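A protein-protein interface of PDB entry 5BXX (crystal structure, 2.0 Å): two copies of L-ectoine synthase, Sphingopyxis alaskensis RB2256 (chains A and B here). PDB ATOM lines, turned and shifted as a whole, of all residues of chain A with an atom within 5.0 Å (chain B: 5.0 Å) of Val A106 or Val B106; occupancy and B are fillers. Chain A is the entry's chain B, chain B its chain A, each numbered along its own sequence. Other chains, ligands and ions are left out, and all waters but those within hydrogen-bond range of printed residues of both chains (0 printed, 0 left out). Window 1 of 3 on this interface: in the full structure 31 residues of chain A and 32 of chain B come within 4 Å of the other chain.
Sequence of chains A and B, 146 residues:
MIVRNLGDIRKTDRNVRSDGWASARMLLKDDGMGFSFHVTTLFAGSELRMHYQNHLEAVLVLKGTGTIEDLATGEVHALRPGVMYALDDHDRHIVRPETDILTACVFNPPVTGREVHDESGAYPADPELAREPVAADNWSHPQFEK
O of Asn B108 sits at hydrogen-bond distance from N of Leu B56 (2.7 Å).
The backbone NH (N) of Leu A56 is in hydrogen-bond range of the backbone carbonyl oxygen (O) of Asn A108 (2.7 Å).
The backbone carbonyl oxygen of Val B106 sits at hydrogen-bond distance from the backbone NH of Ala B58 (2.9 Å).
O of Ala A58 is in hydrogen-bond range of N of Val A106, 2.9 Å away.
Among the printed residues, merely in contact across the chains: Phe A35 with Ala B58, Phe A35 with Val B106, Phe A35 with Asn B108, Phe A37 with Ala B58, Phe A37 with Ala B104, Phe A37 with Val B106, Ala A58 with Phe B35, Ala A58 with Phe B37, Ala A104 with Phe B37, Val A106 with Phe B35, Val A106 with Phe B37, Val A106 with Val B106 and Asn A108 with Phe B35.
Val A106 touches just these residues of chain B: Phe B35, Phe B37 and Val B106.
Val B106 touches three residues of chain A.
Of the printed residues of chain B, Ala A104 touches Phe B37 (3.8 Å).
Printed residues of chain B within 4 Å of Phe A37: Ala B58 (3.8 Å), Ala B104 (3.8 Å) and Val B106 (3.9 Å).
Printed residues of chain A within 4 Å of Phe B37: Ala A58, Ala A104 and Val A106.
Of the printed residues of chain B, Asn A108 touches Phe B35.
The nearest printed residue of chain B that does not touch Val A106 is Ser B36 (6.2 Å).
The nearest printed residue of chain A that does not touch Val B106 is Ser A36 (6.4 Å).
Of the 11 printed residues of chain A, 6 touch a printed residue of chain B.
Hydrophobic or aromatic side chains of chain A that line the printed part of chain B: Phe A35, Phe A37, Ala A58 and Val A106.
Of the 11 printed residues of chain B, 6 touch a printed residue of chain A.
Hydrophobic or aromatic side chains of chain B within 4 Å of the printed part of chain A: Phe B35, Phe B37, Ala B58 and Val B106.
Among the printed residues, 13 pairs touch across the chains.
Phe A35 touches Ala B58, and with the chains exchanged Ala A58 touches Phe B35.
Phe A35 touches Asn B108, and with the chains exchanged Asn A108 touches Phe B35.
Phe A37 touches Ala B58, and with the chains exchanged Ala A58 touches Phe B37.
Phe A37 touches Val B106, and with the chains exchanged Val A106 touches Phe B37.
Of the 13 pairs that touch across the chains among the printed residues, 13 have their exchanged pair printed and touching as well.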
ATOM      1  N   PHE A  35      -3.122 -18.872 -11.822  1.00  0.00           N
ATOM      2  CA  PHE A  35      -2.281 -19.872 -11.168  1.00  0.00           C
ATOM      3  C   PHE A  35      -1.187 -19.103 -10.443  1.00  0.00           C
ATOM      4  O   PHE A  35      -0.923 -17.919 -10.764  1.00  0.00           O
ATOM      5  CB  PHE A  35      -1.668 -20.864 -12.181  1.00  0.00           C
ATOM      6  CG  PHE A  35      -0.918 -20.189 -13.312  1.00  0.00           C
ATOM      7  CD1 PHE A  35      -1.549 -19.881 -14.503  1.00  0.00           C
ATOM      8  CD2 PHE A  35       0.439 -19.886 -13.171  1.00  0.00           C
ATOM      9  CE1 PHE A  35      -0.846 -19.206 -15.573  1.00  0.00           C
ATOM     10  CE2 PHE A  35       1.157 -19.247 -14.221  1.00  0.00           C
ATOM     11  CZ  PHE A  35       0.513 -18.917 -15.420  1.00  0.00           C
ATOM     12  N   SER A  36      -0.527 -19.749  -9.485  1.00  0.00           N
ATOM     13  CA  SER A  36       0.688 -19.175  -8.919  1.00  0.00           C
ATOM     14  C   SER A  36       1.839 -20.010  -9.437  1.00  0.00           C
ATOM     15  O   SER A  36       1.690 -21.161  -9.863  1.00  0.00           O
ATOM     16  CB  SER A  36       0.688 -19.115  -7.383  1.00  0.00           C
ATOM     17  OG  SER A  36       0.541 -20.452  -6.789  1.00  0.00           O
ATOM     18  N   PHE A  37       3.010 -19.427  -9.379  1.00  0.00           N
ATOM     19  CA  PHE A  37       4.208 -19.968 -10.016  1.00  0.00           C
ATOM     20  C   PHE A  37       5.344 -19.697  -9.038  1.00  0.00           C
ATOM     21  O   PHE A  37       5.547 -18.532  -8.623  1.00  0.00           O
ATOM     22  CB  PHE A  37       4.383 -19.261 -11.360  1.00  0.00           C
ATOM     23  CG  PHE A  37       5.292 -19.916 -12.366  1.00  0.00           C
ATOM     24  CD1 PHE A  37       5.769 -21.179 -12.259  1.00  0.00           C
ATOM     25  CD2 PHE A  37       5.664 -19.181 -13.489  1.00  0.00           C
ATOM     26  CE1 PHE A  37       6.583 -21.708 -13.242  1.00  0.00           C
ATOM     27  CE2 PHE A  37       6.466 -19.713 -14.469  1.00  0.00           C
ATOM     28  CZ  PHE A  37       6.945 -20.950 -14.349  1.00  0.00           C
ATOM     29  N   LEU A  56      -4.295 -27.994  -6.824  1.00  0.00           N
ATOM     30  CA  LEU A  56      -3.561 -28.896  -7.700  1.00  0.00           C
ATOM     31  C   LEU A  56      -2.211 -28.305  -7.937  1.00  0.00           C
ATOM     32  O   LEU A  56      -2.098 -27.069  -8.161  1.00  0.00           O
ATOM     33  CB  LEU A  56      -4.309 -29.111  -9.016  1.00  0.00           C
ATOM     34  CG  LEU A  56      -5.759 -29.461  -8.757  1.00  0.00           C
ATOM     35  CD1 LEU A  56      -6.451 -29.464 -10.071  1.00  0.00           C
ATOM     36  CD2 LEU A  56      -5.821 -30.811  -8.065  1.00  0.00           C
ATOM     37  N   GLU A  57      -1.198 -29.167  -7.929  1.00  0.00           N
ATOM     38  CA  GLU A  57       0.176 -28.716  -8.136  1.00  0.00           C
ATOM     39  C   GLU A  57       0.846 -29.518  -9.218  1.00  0.00           C
ATOM     40  O   GLU A  57       0.642 -30.747  -9.344  1.00  0.00           O
ATOM     41  CB  GLU A  57       1.017 -28.795  -6.861  1.00  0.00           C
ATOM     42  CG  GLU A  57       2.345 -28.167  -7.031  1.00  0.00           C
ATOM     43  CD  GLU A  57       3.324 -28.397  -5.911  1.00  0.00           C
ATOM     44  OE1 GLU A  57       3.196 -29.387  -5.187  1.00  0.00           O
ATOM     45  OE2 GLU A  57       4.269 -27.565  -5.792  1.00  0.00           O
ATOM     46  N   ALA A  58       1.603 -28.792 -10.051  1.00  0.00           N
ATOM     47  CA  ALA A  58       2.570 -29.397 -10.951  1.00  0.00           C
ATOM     48  C   ALA A  58       3.988 -28.967 -10.554  1.00  0.00           C
ATOM     49  O   ALA A  58       4.214 -27.806 -10.243  1.00  0.00           O
ATOM     50  CB  ALA A  58       2.286 -29.027 -12.322  1.00  0.00           C
ATOM     51  N   ALA A 104      10.418 -25.942 -10.261  1.00  0.00           N
ATOM     52  CA  ALA A 104       9.418 -24.984 -10.708  1.00  0.00           C
ATOM     53  C   ALA A 104       8.046 -25.549 -10.466  1.00  0.00           C
ATOM     54  O   ALA A 104       7.687 -26.594 -11.047  1.00  0.00           O
ATOM     55  CB  ALA A 104       9.600 -24.655 -12.196  1.00  0.00           C
ATOM     56  N   CYS A 105       7.306 -24.865  -9.604  1.00  0.00           N
ATOM     57  CA  CYS A 105       5.977 -25.271  -9.186  1.00  0.00           C
ATOM     58  C   CYS A 105       4.860 -24.359  -9.644  1.00  0.00           C
ATOM     59  O   CYS A 105       4.966 -23.133  -9.576  1.00  0.00           O
ATOM     60  CB  CYS A 105       5.943 -25.358  -7.648  1.00  0.00           C
ATOM     61  SG  CYS A 105       7.348 -26.271  -6.964  1.00  0.00           S
ATOM     62  N   VAL A 106       3.786 -24.983 -10.108  1.00  0.00           N
ATOM     63  CA  VAL A 106       2.601 -24.308 -10.577  1.00  0.00           C
ATOM     64  C   VAL A 106       1.413 -24.742  -9.711  1.00  0.00           C
ATOM     65  O   VAL A 106       1.153 -25.955  -9.570  1.00  0.00           O
ATOM     66  CB  VAL A 106       2.295 -24.616 -12.043  1.00  0.00           C
ATOM     67  CG1 VAL A 106       1.172 -23.696 -12.523  1.00  0.00           C
ATOM     68  CG2 VAL A 106       3.535 -24.452 -12.958  1.00  0.00           C
ATOM     69  N   PHE A 107       0.712 -23.789  -9.103  1.00  0.00           N
ATOM     70  CA  PHE A 107      -0.510 -24.118  -8.312  1.00  0.00           C
ATOM     71  C   PHE A 107      -1.775 -23.520  -8.893  1.00  0.00           C
ATOM     72  O   PHE A 107      -1.757 -22.372  -9.383  1.00  0.00           O
ATOM     73  CB  PHE A 107      -0.399 -23.618  -6.888  1.00  0.00           C
ATOM     74  CG  PHE A 107       0.608 -24.354  -6.035  1.00  0.00           C
ATOM     75  CD1 PHE A 107       0.214 -25.434  -5.236  1.00  0.00           C
ATOM     76  CD2 PHE A 107       1.932 -23.950  -5.996  1.00  0.00           C
ATOM     77  CE1 PHE A 107       1.127 -26.077  -4.434  1.00  0.00           C
ATOM     78  CE2 PHE A 107       2.852 -24.603  -5.192  1.00  0.00           C
ATOM     79  CZ  PHE A 107       2.445 -25.660  -4.405  1.00  0.00           C
ATOM     80  N   ASN A 108      -2.827 -24.337  -8.934  1.00  0.00           N
ATOM     81  CA  ASN A 108      -4.208 -23.961  -9.300  1.00  0.00           C
ATOM     82  C   ASN A 108      -5.199 -24.554  -8.295  1.00  0.00           C
ATOM     83  O   ASN A 108      -5.160 -25.759  -8.033  1.00  0.00           O
ATOM     84  CB  ASN A 108      -4.551 -24.451 -10.682  1.00  0.00           C
ATOM     85  CG  ASN A 108      -5.810 -23.814 -11.251  1.00  0.00           C
ATOM     86  OD1 ASN A 108      -6.298 -22.795 -10.774  1.00  0.00           O
ATOM     87  ND2 ASN A 108      -6.334 -24.421 -12.289  1.00  0.00           N
ATOM     88  N   PHE B  35      -4.485 -25.742 -16.408  1.00  0.00           N
ATOM     89  CA  PHE B  35      -3.400 -25.071 -17.080  1.00  0.00           C
ATOM     90  C   PHE B  35      -2.595 -26.130 -17.796  1.00  0.00           C
ATOM     91  O   PHE B  35      -2.611 -27.314 -17.414  1.00  0.00           O
ATOM     92  CB  PHE B  35      -2.510 -24.320 -16.084  1.00  0.00           C
ATOM     93  CG  PHE B  35      -1.839 -25.221 -15.006  1.00  0.00           C
ATOM     94  CD1 PHE B  35      -2.416 -25.369 -13.735  1.00  0.00           C
ATOM     95  CD2 PHE B  35      -0.625 -25.863 -15.245  1.00  0.00           C
ATOM     96  CE1 PHE B  35      -1.796 -26.172 -12.733  1.00  0.00           C
ATOM     97  CE2 PHE B  35      -0.002 -26.679 -14.256  1.00  0.00           C
ATOM     98  CZ  PHE B  35      -0.586 -26.818 -13.002  1.00  0.00           C
ATOM     99  N   SER B  36      -1.890 -25.727 -18.834  1.00  0.00           N
ATOM    100  CA  SER B  36      -0.898 -26.597 -19.464  1.00  0.00           C
ATOM    101  C   SER B  36       0.523 -26.137 -19.004  1.00  0.00           C
ATOM    102  O   SER B  36       0.672 -25.028 -18.507  1.00  0.00           O
ATOM    103  CB  SER B  36      -1.056 -26.599 -20.990  1.00  0.00           C
ATOM    104  OG  SER B  36      -0.925 -25.289 -21.570  1.00  0.00           O
ATOM    105  N   PHE B  37       1.533 -27.004 -19.177  1.00  0.00           N
ATOM    106  CA  PHE B  37       2.870 -26.870 -18.602  1.00  0.00           C
ATOM    107  C   PHE B  37       3.857 -27.453 -19.631  1.00  0.00           C
ATOM    108  O   PHE B  37       3.739 -28.637 -20.048  1.00  0.00           O
ATOM    109  CB  PHE B  37       2.949 -27.615 -17.270  1.00  0.00           C
ATOM    110  CG  PHE B  37       4.145 -27.280 -16.373  1.00  0.00           C
ATOM    111  CD1 PHE B  37       4.853 -26.080 -16.467  1.00  0.00           C
ATOM    112  CD2 PHE B  37       4.515 -28.181 -15.365  1.00  0.00           C
ATOM    113  CE1 PHE B  37       5.914 -25.805 -15.590  1.00  0.00           C
ATOM    114  CE2 PHE B  37       5.550 -27.896 -14.481  1.00  0.00           C
ATOM    115  CZ  PHE B  37       6.256 -26.696 -14.606  1.00  0.00           C
ATOM    116  N   LEU B  56      -3.356 -16.626 -21.051  1.00  0.00           N
ATOM    117  CA  LEU B  56      -2.333 -15.982 -20.249  1.00  0.00           C
ATOM    118  C   LEU B  56      -1.174 -16.954 -20.143  1.00  0.00           C
ATOM    119  O   LEU B  56      -1.394 -18.176 -19.819  1.00  0.00           O
ATOM    120  CB  LEU B  56      -2.858 -15.609 -18.870  1.00  0.00           C
ATOM    121  CG  LEU B  56      -4.110 -14.733 -18.909  1.00  0.00           C
ATOM    122  CD1 LEU B  56      -4.630 -14.564 -17.510  1.00  0.00           C
ATOM    123  CD2 LEU B  56      -3.854 -13.316 -19.621  1.00  0.00           C
ATOM    124  N   GLU B  57       0.036 -16.445 -20.386  1.00  0.00           N
ATOM    125  CA  GLU B  57       1.262 -17.257 -20.297  1.00  0.00           C
ATOM    126  C   GLU B  57       2.269 -16.680 -19.326  1.00  0.00           C
ATOM    127  O   GLU B  57       2.512 -15.450 -19.285  1.00  0.00           O
ATOM    128  CB  GLU B  57       1.942 -17.416 -21.653  1.00  0.00           C
ATOM    129  CG  GLU B  57       3.180 -18.371 -21.589  1.00  0.00           C
ATOM    130  CD  GLU B  57       4.053 -18.326 -22.825  1.00  0.00           C
ATOM    131  OE1 GLU B  57       4.030 -17.283 -23.507  1.00  0.00           O
ATOM    132  OE2 GLU B  57       4.817 -19.308 -23.082  1.00  0.00           O
ATOM    133  N   ALA B  58       2.804 -17.568 -18.498  1.00  0.00           N
ATOM    134  CA  ALA B  58       3.949 -17.239 -17.687  1.00  0.00           C
ATOM    135  C   ALA B  58       5.154 -18.074 -18.161  1.00  0.00           C
ATOM    136  O   ALA B  58       5.015 -19.230 -18.538  1.00  0.00           O
ATOM    137  CB  ALA B  58       3.637 -17.500 -16.274  1.00  0.00           C
ATOM    138  N   ALA B 104      10.517 -22.877 -18.893  1.00  0.00           N
ATOM    139  CA  ALA B 104       9.329 -23.570 -18.387  1.00  0.00           C
ATOM    140  C   ALA B 104       8.199 -22.574 -18.481  1.00  0.00           C
ATOM    141  O   ALA B 104       8.291 -21.466 -17.883  1.00  0.00           O
ATOM    142  CB  ALA B 104       9.520 -24.023 -16.964  1.00  0.00           C
ATOM    143  N   CYS B 105       7.185 -22.987 -19.234  1.00  0.00           N
ATOM    144  CA  CYS B 105       5.995 -22.237 -19.625  1.00  0.00           C
ATOM    145  C   CYS B 105       4.705 -22.785 -19.044  1.00  0.00           C
ATOM    146  O   CYS B 105       4.491 -24.034 -19.094  1.00  0.00           O
ATOM    147  CB  CYS B 105       5.786 -22.305 -21.141  1.00  0.00           C
ATOM    148  SG  CYS B 105       7.121 -21.940 -22.104  1.00  0.00           S
ATOM    149  N   VAL B 106       3.825 -21.867 -18.627  1.00  0.00           N
ATOM    150  CA  VAL B 106       2.495 -22.158 -18.117  1.00  0.00           C
ATOM    151  C   VAL B 106       1.464 -21.358 -18.907  1.00  0.00           C
ATOM    152  O   VAL B 106       1.571 -20.116 -19.060  1.00  0.00           O
ATOM    153  CB  VAL B 106       2.359 -21.813 -16.632  1.00  0.00           C
ATOM    154  CG1 VAL B 106       1.077 -22.420 -16.105  1.00  0.00           C
ATOM    155  CG2 VAL B 106       3.588 -22.333 -15.826  1.00  0.00           C
ATOM    156  N   PHE B 107       0.484 -22.058 -19.432  1.00  0.00           N
ATOM    157  CA  PHE B 107      -0.643 -21.435 -20.110  1.00  0.00           C
ATOM    158  C   PHE B 107      -1.947 -21.660 -19.363  1.00  0.00           C
ATOM    159  O   PHE B 107      -2.275 -22.779 -18.922  1.00  0.00           O
ATOM    160  CB  PHE B 107      -0.789 -21.974 -21.515  1.00  0.00           C
ATOM    161  CG  PHE B 107       0.218 -21.491 -22.474  1.00  0.00           C
ATOM    162  CD1 PHE B 107       0.003 -20.319 -23.188  1.00  0.00           C
ATOM    163  CD2 PHE B 107       1.371 -22.226 -22.716  1.00  0.00           C
ATOM    164  CE1 PHE B 107       0.922 -19.880 -24.111  1.00  0.00           C
ATOM    165  CE2 PHE B 107       2.302 -21.775 -23.622  1.00  0.00           C
ATOM    166  CZ  PHE B 107       2.073 -20.590 -24.331  1.00  0.00           C
ATOM    167  N   ASN B 108      -2.679 -20.584 -19.214  1.00  0.00           N
ATOM    168  CA  ASN B 108      -4.050 -20.611 -18.783  1.00  0.00           C
ATOM    169  C   ASN B 108      -4.994 -19.882 -19.713  1.00  0.00           C
ATOM    170  O   ASN B 108      -4.828 -18.652 -19.927  1.00  0.00           O
ATOM    171  CB  ASN B 108      -4.182 -19.978 -17.433  1.00  0.00           C
ATOM    172  CG  ASN B 108      -5.629 -19.877 -17.011  1.00  0.00           C
ATOM    173  OD1 ASN B 108      -6.444 -20.702 -17.377  1.00  0.00           O
ATOM    174  ND2 ASN B 108      -5.947 -18.879 -16.235  1.00  0.00           N
